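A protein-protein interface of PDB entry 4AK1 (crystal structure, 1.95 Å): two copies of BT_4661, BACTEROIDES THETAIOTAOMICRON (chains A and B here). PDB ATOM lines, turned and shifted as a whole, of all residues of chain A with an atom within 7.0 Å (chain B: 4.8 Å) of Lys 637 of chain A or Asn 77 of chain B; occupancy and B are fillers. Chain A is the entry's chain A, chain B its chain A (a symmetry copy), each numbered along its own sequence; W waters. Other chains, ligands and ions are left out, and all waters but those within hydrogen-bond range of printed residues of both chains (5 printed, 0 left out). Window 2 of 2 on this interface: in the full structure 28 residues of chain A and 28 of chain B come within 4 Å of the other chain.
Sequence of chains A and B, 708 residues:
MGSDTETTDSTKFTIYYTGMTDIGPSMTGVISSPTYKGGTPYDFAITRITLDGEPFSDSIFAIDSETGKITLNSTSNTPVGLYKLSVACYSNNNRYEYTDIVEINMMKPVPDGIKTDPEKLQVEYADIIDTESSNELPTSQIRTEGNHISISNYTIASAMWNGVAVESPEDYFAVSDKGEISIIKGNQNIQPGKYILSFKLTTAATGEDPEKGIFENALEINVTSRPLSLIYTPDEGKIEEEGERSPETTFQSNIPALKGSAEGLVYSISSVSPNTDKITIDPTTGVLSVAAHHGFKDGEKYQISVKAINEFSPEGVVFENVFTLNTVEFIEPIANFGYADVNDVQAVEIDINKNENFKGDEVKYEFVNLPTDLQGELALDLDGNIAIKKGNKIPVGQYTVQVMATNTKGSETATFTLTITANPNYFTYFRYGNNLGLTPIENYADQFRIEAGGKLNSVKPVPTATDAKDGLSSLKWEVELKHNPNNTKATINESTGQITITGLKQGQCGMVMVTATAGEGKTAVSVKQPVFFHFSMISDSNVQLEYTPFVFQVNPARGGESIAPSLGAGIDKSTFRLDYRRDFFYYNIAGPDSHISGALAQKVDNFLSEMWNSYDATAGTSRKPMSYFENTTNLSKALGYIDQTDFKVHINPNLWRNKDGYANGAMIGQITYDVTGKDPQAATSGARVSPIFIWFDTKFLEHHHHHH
Water W5 bridges the backbone carbonyl oxygen of Lys 637 of chain A (2.6 Å) and the side-chain amide oxygen of Asn 77 of chain B (3.0 Å). Water W3 lies within hydrogen-bond range of OD2 of Asp 58 of chain B, O of Pro 653 of chain A and ND2 of Asn 77 of chain B. Water W4 lies within hydrogen-bond range of the backbone carbonyl oxygen (O) of Ser 636 of chain A (2.8 Å) and the side-chain amide nitrogen (ND2) of Asn 77 of chain B (3.3 Å). Water W1 lies within hydrogen-bond range of the side-chain amide nitrogen of Asn 634 of chain A (2.8 Å) and the backbone carbonyl oxygen of Thr 75 of chain B (2.9 Å). Water W2 lies within hydrogen-bond range of the side-chain hydroxyl of Ser 636 of chain A, the backbone carbonyl oxygen of Thr 75 of chain B and the side-chain amino group of Lys 637 of chain A.
Hydrophobic or aromatic side chains of chain B within 4 Å of the printed part of chain A: Pro 79. Of the 15 printed residues of chain A, 3 touch a printed residue of chain B. Hydrophobic or aromatic side chains of chain A within 4 Å of the printed part of chain B: Leu 655. Along chain A the printed residues that touch a printed residue of chain B span positions 636 to 655. Among the printed residues, no Asp or Glu carboxylate lies within 4 Å of a Lys or Arg side-chain nitrogen of the other chain.
No position is printed for both chains.
The backbone carbonyl oxygen (O) of Ser 636 of chain A is in hydrogen-bond range of the side-chain amide nitrogen (ND2) of Asn 652 of chain A, at 3.4 Å. OD1 of Asn 634 of chain A is in hydrogen-bond range of OG of Ser 636 of chain A (2.6 Å).
Leu 635 of chain A touches none of the printed residues of chain B. Of chain B, only Thr 75, Ser 76 and Asn 77 come within 4 Å of Lys 637 of chain A. Ala 638 of chain A touches none of the printed residues of chain B. Of the printed residues of chain B, Leu 655 of chain A touches Asn 77 and Pro 79. Printed residues of chain A within 4 Å of Thr 75 of chain B: Lys 637. Printed residues of chain A within 4 Å of Ser 76 of chain B: Lys 637. The nearest printed residue of chain B that does not touch Leu 655 of chain A is Thr 78 of chain B (5.6 Å).
Among the printed residues, pairs that only touch across the chains: Lys 637 of chain A with Ser 76 of chain B (3.6 Å), Leu 655 of chain A with Asn 77 of chain B (3.9 Å) and Leu 655 of chain A with Pro 79 of chain B (3.98 Å).
NZ of Lys 637 of chain A lies close to OD1 of Asn 77 of chain B, at 3.3 Å. The backbone carbonyl oxygen (O) of Ser 636 of chain A is in hydrogen-bond range of the side-chain amide nitrogen (ND2) of Asn 77 of chain B, 2.9 Å away. The side-chain amino group of Lys 637 of chain A lies within hydrogen-bond range of the backbone carbonyl oxygen of Thr 75 of chain B.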
ATOM      1  N   SER A 614     -10.893  15.213  -0.040  1.00  0.00           N
ATOM      2  CA  SER A 614     -11.128  15.411   1.395  1.00  0.00           C
ATOM      3  C   SER A 614     -11.527  16.865   1.680  1.00  0.00           C
ATOM      4  O   SER A 614     -12.242  17.146   2.645  1.00  0.00           O
ATOM      5  CB  SER A 614      -9.924  14.979   2.237  1.00  0.00           C
ATOM      6  OG  SER A 614      -8.880  15.941   2.178  1.00  0.00           O
ATOM      7  N   TYR A 615     -11.083  17.782   0.827  1.00  0.00           N
ATOM      8  CA  TYR A 615     -11.482  19.174   0.958  1.00  0.00           C
ATOM      9  C   TYR A 615     -12.911  19.344   0.441  1.00  0.00           C
ATOM     10  O   TYR A 615     -13.759  19.870   1.138  1.00  0.00           O
ATOM     11  CB  TYR A 615     -10.494  20.107   0.239  1.00  0.00           C
ATOM     12  CG  TYR A 615     -10.960  21.533   0.108  1.00  0.00           C
ATOM     13  CD1 TYR A 615     -10.710  22.464   1.116  1.00  0.00           C
ATOM     14  CD2 TYR A 615     -11.656  21.961  -1.038  1.00  0.00           C
ATOM     15  CE1 TYR A 615     -11.131  23.779   0.993  1.00  0.00           C
ATOM     16  CE2 TYR A 615     -12.089  23.269  -1.166  1.00  0.00           C
ATOM     17  CZ  TYR A 615     -11.817  24.180  -0.151  1.00  0.00           C
ATOM     18  OH  TYR A 615     -12.250  25.481  -0.275  1.00  0.00           O
ATOM     19  N   LYS A 624      -8.568  25.574  -5.332  1.00  0.00           N
ATOM     20  CA  LYS A 624      -9.385  25.819  -4.124  1.00  0.00           C
ATOM     21  C   LYS A 624      -8.832  25.263  -2.789  1.00  0.00           C
ATOM     22  O   LYS A 624      -8.771  26.014  -1.819  1.00  0.00           O
ATOM     23  CB  LYS A 624     -10.836  25.361  -4.318  1.00  0.00           C
ATOM     24  CG  LYS A 624     -11.643  26.208  -5.267  1.00  0.00           C
ATOM     25  CD  LYS A 624     -13.127  25.891  -5.124  1.00  0.00           C
ATOM     26  CE  LYS A 624     -13.958  27.045  -5.666  1.00  0.00           C
ATOM     27  NZ  LYS A 624     -14.265  26.861  -7.112  1.00  0.00           N
ATOM     28  N   PRO A 625      -8.430  23.967  -2.732  1.00  0.00           N
ATOM     29  CA  PRO A 625      -7.982  23.412  -1.441  1.00  0.00           C
ATOM     30  C   PRO A 625      -6.716  24.067  -0.862  1.00  0.00           C
ATOM     31  O   PRO A 625      -6.429  23.896   0.331  1.00  0.00           O
ATOM     32  CB  PRO A 625      -7.686  21.943  -1.774  1.00  0.00           C
ATOM     33  CG  PRO A 625      -8.491  21.659  -3.018  1.00  0.00           C
ATOM     34  CD  PRO A 625      -8.372  22.940  -3.792  1.00  0.00           C
ATOM     35  N   ASN A 631     -10.865  30.747   0.191  1.00  0.00           N
ATOM     36  CA  ASN A 631     -11.250  30.302   1.549  1.00  0.00           C
ATOM     37  C   ASN A 631     -11.308  31.429   2.593  1.00  0.00           C
ATOM     38  O   ASN A 631     -11.216  31.165   3.806  1.00  0.00           O
ATOM     39  CB  ASN A 631     -10.297  29.192   2.026  1.00  0.00           C
ATOM     40  CG  ASN A 631     -10.470  27.900   1.250  1.00  0.00           C
ATOM     41  OD1 ASN A 631     -11.442  27.189   1.455  1.00  0.00           O
ATOM     42  ND2 ASN A 631      -9.532  27.601   0.347  1.00  0.00           N
ATOM     43  N   ASN A 634     -13.604  31.102   5.639  1.00  0.00           N
ATOM     44  CA  ASN A 634     -13.193  30.105   6.627  1.00  0.00           C
ATOM     45  C   ASN A 634     -11.885  29.417   6.266  1.00  0.00           C
ATOM     46  O   ASN A 634     -11.867  28.341   5.660  1.00  0.00           O
ATOM     47  CB  ASN A 634     -14.305  29.086   6.910  1.00  0.00           C
ATOM     48  CG  ASN A 634     -14.019  28.247   8.150  1.00  0.00           C
ATOM     49  OD1 ASN A 634     -12.904  28.281   8.691  1.00  0.00           O
ATOM     50  ND2 ASN A 634     -15.025  27.499   8.613  1.00  0.00           N
ATOM     51  N   LEU A 635     -10.782  30.053   6.655  1.00  0.00           N
ATOM     52  CA  LEU A 635      -9.452  29.572   6.276  1.00  0.00           C
ATOM     53  C   LEU A 635      -9.105  28.206   6.885  1.00  0.00           C
ATOM     54  O   LEU A 635      -8.325  27.458   6.318  1.00  0.00           O
ATOM     55  CB  LEU A 635      -8.373  30.603   6.610  1.00  0.00           C
ATOM     56  CG  LEU A 635      -8.299  31.857   5.727  1.00  0.00           C
ATOM     57  CD1 LEU A 635      -7.415  32.922   6.380  1.00  0.00           C
ATOM     58  CD2 LEU A 635      -7.784  31.517   4.335  1.00  0.00           C
ATOM     59  N   SER A 636      -9.714  27.889   8.024  1.00  0.00           N
ATOM     60  CA  SER A 636      -9.467  26.606   8.694  1.00  0.00           C
ATOM     61  C   SER A 636      -9.872  25.389   7.819  1.00  0.00           C
ATOM     62  O   SER A 636      -9.416  24.274   8.052  1.00  0.00           O
ATOM     63  CB  SER A 636     -10.162  26.576  10.068  1.00  0.00           C
ATOM     64  OG  SER A 636     -11.562  26.385   9.938  1.00  0.00           O
ATOM     65  N   LYS A 637     -10.691  25.620   6.786  1.00  0.00           N
ATOM     66  CA  LYS A 637     -11.100  24.541   5.884  1.00  0.00           C
ATOM     67  C   LYS A 637     -10.059  24.195   4.825  1.00  0.00           C
ATOM     68  O   LYS A 637     -10.056  23.083   4.311  1.00  0.00           O
ATOM     69  CB  LYS A 637     -12.450  24.856   5.210  1.00  0.00           C
ATOM     70  CG  LYS A 637     -13.623  25.055   6.170  1.00  0.00           C
ATOM     71  CD  LYS A 637     -13.762  23.876   7.118  1.00  0.00           C
ATOM     72  CE  LYS A 637     -15.198  23.575   7.486  1.00  0.00           C
ATOM     73  NZ  LYS A 637     -15.268  22.294   8.261  1.00  0.00           N
ATOM     74  N   ALA A 638      -9.175  25.136   4.498  1.00  0.00           N
ATOM     75  CA  ALA A 638      -8.145  24.881   3.489  1.00  0.00           C
ATOM     76  C   ALA A 638      -7.169  23.793   3.960  1.00  0.00           C
ATOM     77  O   ALA A 638      -6.941  23.629   5.172  1.00  0.00           O
ATOM     78  CB  ALA A 638      -7.388  26.167   3.160  1.00  0.00           C
ATOM     79  N   LEU A 639      -6.616  23.049   3.010  1.00  0.00           N
ATOM     80  CA  LEU A 639      -5.493  22.149   3.297  1.00  0.00           C
ATOM     81  C   LEU A 639      -4.272  22.989   3.663  1.00  0.00           C
ATOM     82  O   LEU A 639      -3.448  22.587   4.491  1.00  0.00           O
ATOM     83  CB  LEU A 639      -5.164  21.290   2.079  1.00  0.00           C
ATOM     84  CG  LEU A 639      -6.344  20.471   1.546  1.00  0.00           C
ATOM     85  CD1 LEU A 639      -5.881  19.594   0.392  1.00  0.00           C
ATOM     86  CD2 LEU A 639      -6.983  19.635   2.660  1.00  0.00           C
ATOM     87  N   GLY A 640      -4.191  24.164   3.050  1.00  0.00           N
ATOM     88  CA  GLY A 640      -3.098  25.088   3.262  1.00  0.00           C
ATOM     89  C   GLY A 640      -3.382  26.360   2.486  1.00  0.00           C
ATOM     90  O   GLY A 640      -4.301  26.414   1.676  1.00  0.00           O
ATOM     91  N   ASN A 652      -2.668  23.583   7.549  1.00  0.00           N
ATOM     92  CA  ASN A 652      -3.646  23.401   8.621  1.00  0.00           C
ATOM     93  C   ASN A 652      -3.488  22.028   9.302  1.00  0.00           C
ATOM     94  O   ASN A 652      -3.075  21.061   8.649  1.00  0.00           O
ATOM     95  CB  ASN A 652      -5.074  23.609   8.092  1.00  0.00           C
ATOM     96  CG  ASN A 652      -5.465  25.082   8.043  1.00  0.00           C
ATOM     97  OD1 ASN A 652      -4.985  25.879   8.854  1.00  0.00           O
ATOM     98  ND2 ASN A 652      -6.344  25.451   7.105  1.00  0.00           N
ATOM     99  N   PRO A 653      -3.839  21.939  10.601  1.00  0.00           N
ATOM    100  CA  PRO A 653      -3.550  20.715  11.369  1.00  0.00           C
ATOM    101  C   PRO A 653      -4.382  19.475  11.037  1.00  0.00           C
ATOM    102  O   PRO A 653      -5.589  19.566  10.801  1.00  0.00           O
ATOM    103  CB  PRO A 653      -3.821  21.144  12.819  1.00  0.00           C
ATOM    104  CG  PRO A 653      -4.784  22.293  12.715  1.00  0.00           C
ATOM    105  CD  PRO A 653      -4.343  23.028  11.465  1.00  0.00           C
ATOM    106  N   LEU A 655      -4.836  17.432   8.606  1.00  0.00           N
ATOM    107  CA  LEU A 655      -5.519  17.179   7.316  1.00  0.00           C
ATOM    108  C   LEU A 655      -4.693  16.346   6.340  1.00  0.00           C
ATOM    109  O   LEU A 655      -5.239  15.544   5.572  1.00  0.00           O
ATOM    110  CB  LEU A 655      -5.942  18.508   6.654  1.00  0.00           C
ATOM    111  CG  LEU A 655      -6.875  19.397   7.485  1.00  0.00           C
ATOM    112  CD1 LEU A 655      -7.219  20.685   6.734  1.00  0.00           C
ATOM    113  CD2 LEU A 655      -8.126  18.613   7.884  1.00  0.00           C
ATOM    114  N   PHE B  56      -4.673  16.184  18.174  1.00  0.00           N
ATOM    115  CA  PHE B  56      -5.643  16.753  17.249  1.00  0.00           C
ATOM    116  C   PHE B  56      -6.073  18.115  17.798  1.00  0.00           C
ATOM    117  O   PHE B  56      -6.710  18.206  18.848  1.00  0.00           O
ATOM    118  CB  PHE B  56      -6.843  15.817  17.069  1.00  0.00           C
ATOM    119  CG  PHE B  56      -7.791  16.257  15.996  1.00  0.00           C
ATOM    120  CD1 PHE B  56      -7.595  15.861  14.673  1.00  0.00           C
ATOM    121  CD2 PHE B  56      -8.877  17.087  16.295  1.00  0.00           C
ATOM    122  CE1 PHE B  56      -8.462  16.270  13.677  1.00  0.00           C
ATOM    123  CE2 PHE B  56      -9.738  17.510  15.292  1.00  0.00           C
ATOM    124  CZ  PHE B  56      -9.534  17.091  13.986  1.00  0.00           C
ATOM    125  N   ASP B  58      -8.178  20.779  16.638  1.00  0.00           N
ATOM    126  CA  ASP B  58      -9.518  21.366  16.561  1.00  0.00           C
ATOM    127  C   ASP B  58     -10.521  20.694  17.498  1.00  0.00           C
ATOM    128  O   ASP B  58     -10.378  19.526  17.845  1.00  0.00           O
ATOM    129  CB  ASP B  58     -10.038  21.321  15.116  1.00  0.00           C
ATOM    130  CG  ASP B  58      -9.189  22.156  14.142  1.00  0.00           C
ATOM    131  OD1 ASP B  58      -8.397  23.034  14.567  1.00  0.00           O
ATOM    132  OD2 ASP B  58      -9.320  21.936  12.922  1.00  0.00           O
ATOM    133  N   ILE B  60     -13.258  18.972  17.542  1.00  0.00           N
ATOM    134  CA  ILE B  60     -14.123  18.137  16.705  1.00  0.00           C
ATOM    135  C   ILE B  60     -15.308  17.508  17.470  1.00  0.00           C
ATOM    136  O   ILE B  60     -16.421  17.441  16.945  1.00  0.00           O
ATOM    137  CB  ILE B  60     -13.301  17.060  15.938  1.00  0.00           C
ATOM    138  CG1 ILE B  60     -14.201  16.246  14.993  1.00  0.00           C
ATOM    139  CG2 ILE B  60     -12.482  16.190  16.897  1.00  0.00           C
ATOM    140  CD1 ILE B  60     -13.491  15.161  14.205  1.00  0.00           C
ATOM    141  N   THR B  75     -19.275  21.985  12.510  1.00  0.00           N
ATOM    142  CA  THR B  75     -18.452  22.909  11.707  1.00  0.00           C
ATOM    143  C   THR B  75     -16.989  22.447  11.590  1.00  0.00           C
ATOM    144  O   THR B  75     -16.220  23.004  10.802  1.00  0.00           O
ATOM    145  CB  THR B  75     -18.524  24.360  12.223  1.00  0.00           C
ATOM    146  OG1 THR B  75     -17.996  24.419  13.554  1.00  0.00           O
ATOM    147  N   SER B  76     -16.627  21.417  12.355  1.00  0.00           N
ATOM    148  CA  SER B  76     -15.248  20.937  12.425  1.00  0.00           C
ATOM    149  C   SER B  76     -14.813  20.160  11.177  1.00  0.00           C
ATOM    150  O   SER B  76     -15.624  19.481  10.539  1.00  0.00           O
ATOM    151  CB  SER B  76     -15.069  20.057  13.663  1.00  0.00           C
ATOM    152  OG  SER B  76     -13.716  19.658  13.830  1.00  0.00           O
ATOM    153  N   ASN B  77     -13.531  20.266  10.831  1.00  0.00           N
ATOM    154  CA  ASN B  77     -12.930  19.325   9.888  1.00  0.00           C
ATOM    155  C   ASN B  77     -12.989  17.919  10.463  1.00  0.00           C
ATOM    156  O   ASN B  77     -12.871  17.723  11.678  1.00  0.00           O
ATOM    157  CB  ASN B  77     -11.480  19.686   9.568  1.00  0.00           C
ATOM    158  CG  ASN B  77     -11.349  21.030   8.884  1.00  0.00           C
ATOM    159  OD1 ASN B  77     -12.146  21.389   8.010  1.00  0.00           O
ATOM    160  ND2 ASN B  77     -10.320  21.779   9.266  1.00  0.00           N
ATOM    161  N   THR B  78     -13.171  16.941   9.586  1.00  0.00           N
ATOM    162  CA  THR B  78     -13.322  15.546  10.019  1.00  0.00           C
ATOM    163  C   THR B  78     -12.433  14.580   9.224  1.00  0.00           C
ATOM    164  O   THR B  78     -12.944  13.768   8.446  1.00  0.00           O
ATOM    165  CB  THR B  78     -14.795  15.088   9.900  1.00  0.00           C
ATOM    166  OG1 THR B  78     -15.235  15.267   8.550  1.00  0.00           O
ATOM    167  CG2 THR B  78     -15.687  15.894  10.831  1.00  0.00           C
ATOM    168  N   PRO B  79     -11.101  14.666   9.409  1.00  0.00           N
ATOM    169  CA  PRO B  79     -10.230  13.696   8.731  1.00  0.00           C
ATOM    170  C   PRO B  79     -10.477  12.266   9.200  1.00  0.00           C
ATOM    171  O   PRO B  79     -10.953  12.043  10.319  1.00  0.00           O
ATOM    172  CB  PRO B  79      -8.801  14.137   9.107  1.00  0.00           C
ATOM    173  CG  PRO B  79      -8.937  15.333   9.987  1.00  0.00           C
ATOM    174  CD  PRO B  79     -10.369  15.537  10.351  1.00  0.00           C
HETATM  175  O   HOH W   1     -15.246  25.691  10.747  1.00  0.00           O
HETATM  176  O   HOH W   2     -13.052  23.914  10.374  1.00  0.00           O
HETATM  177  O   HOH W   3      -7.898  21.076  10.889  1.00  0.00           O
HETATM  178  O   HOH W   4      -7.754  23.695  10.208  1.00  0.00           O
HETATM  179  O   HOH W   5     -11.372  20.977   5.101  1.00  0.00           O
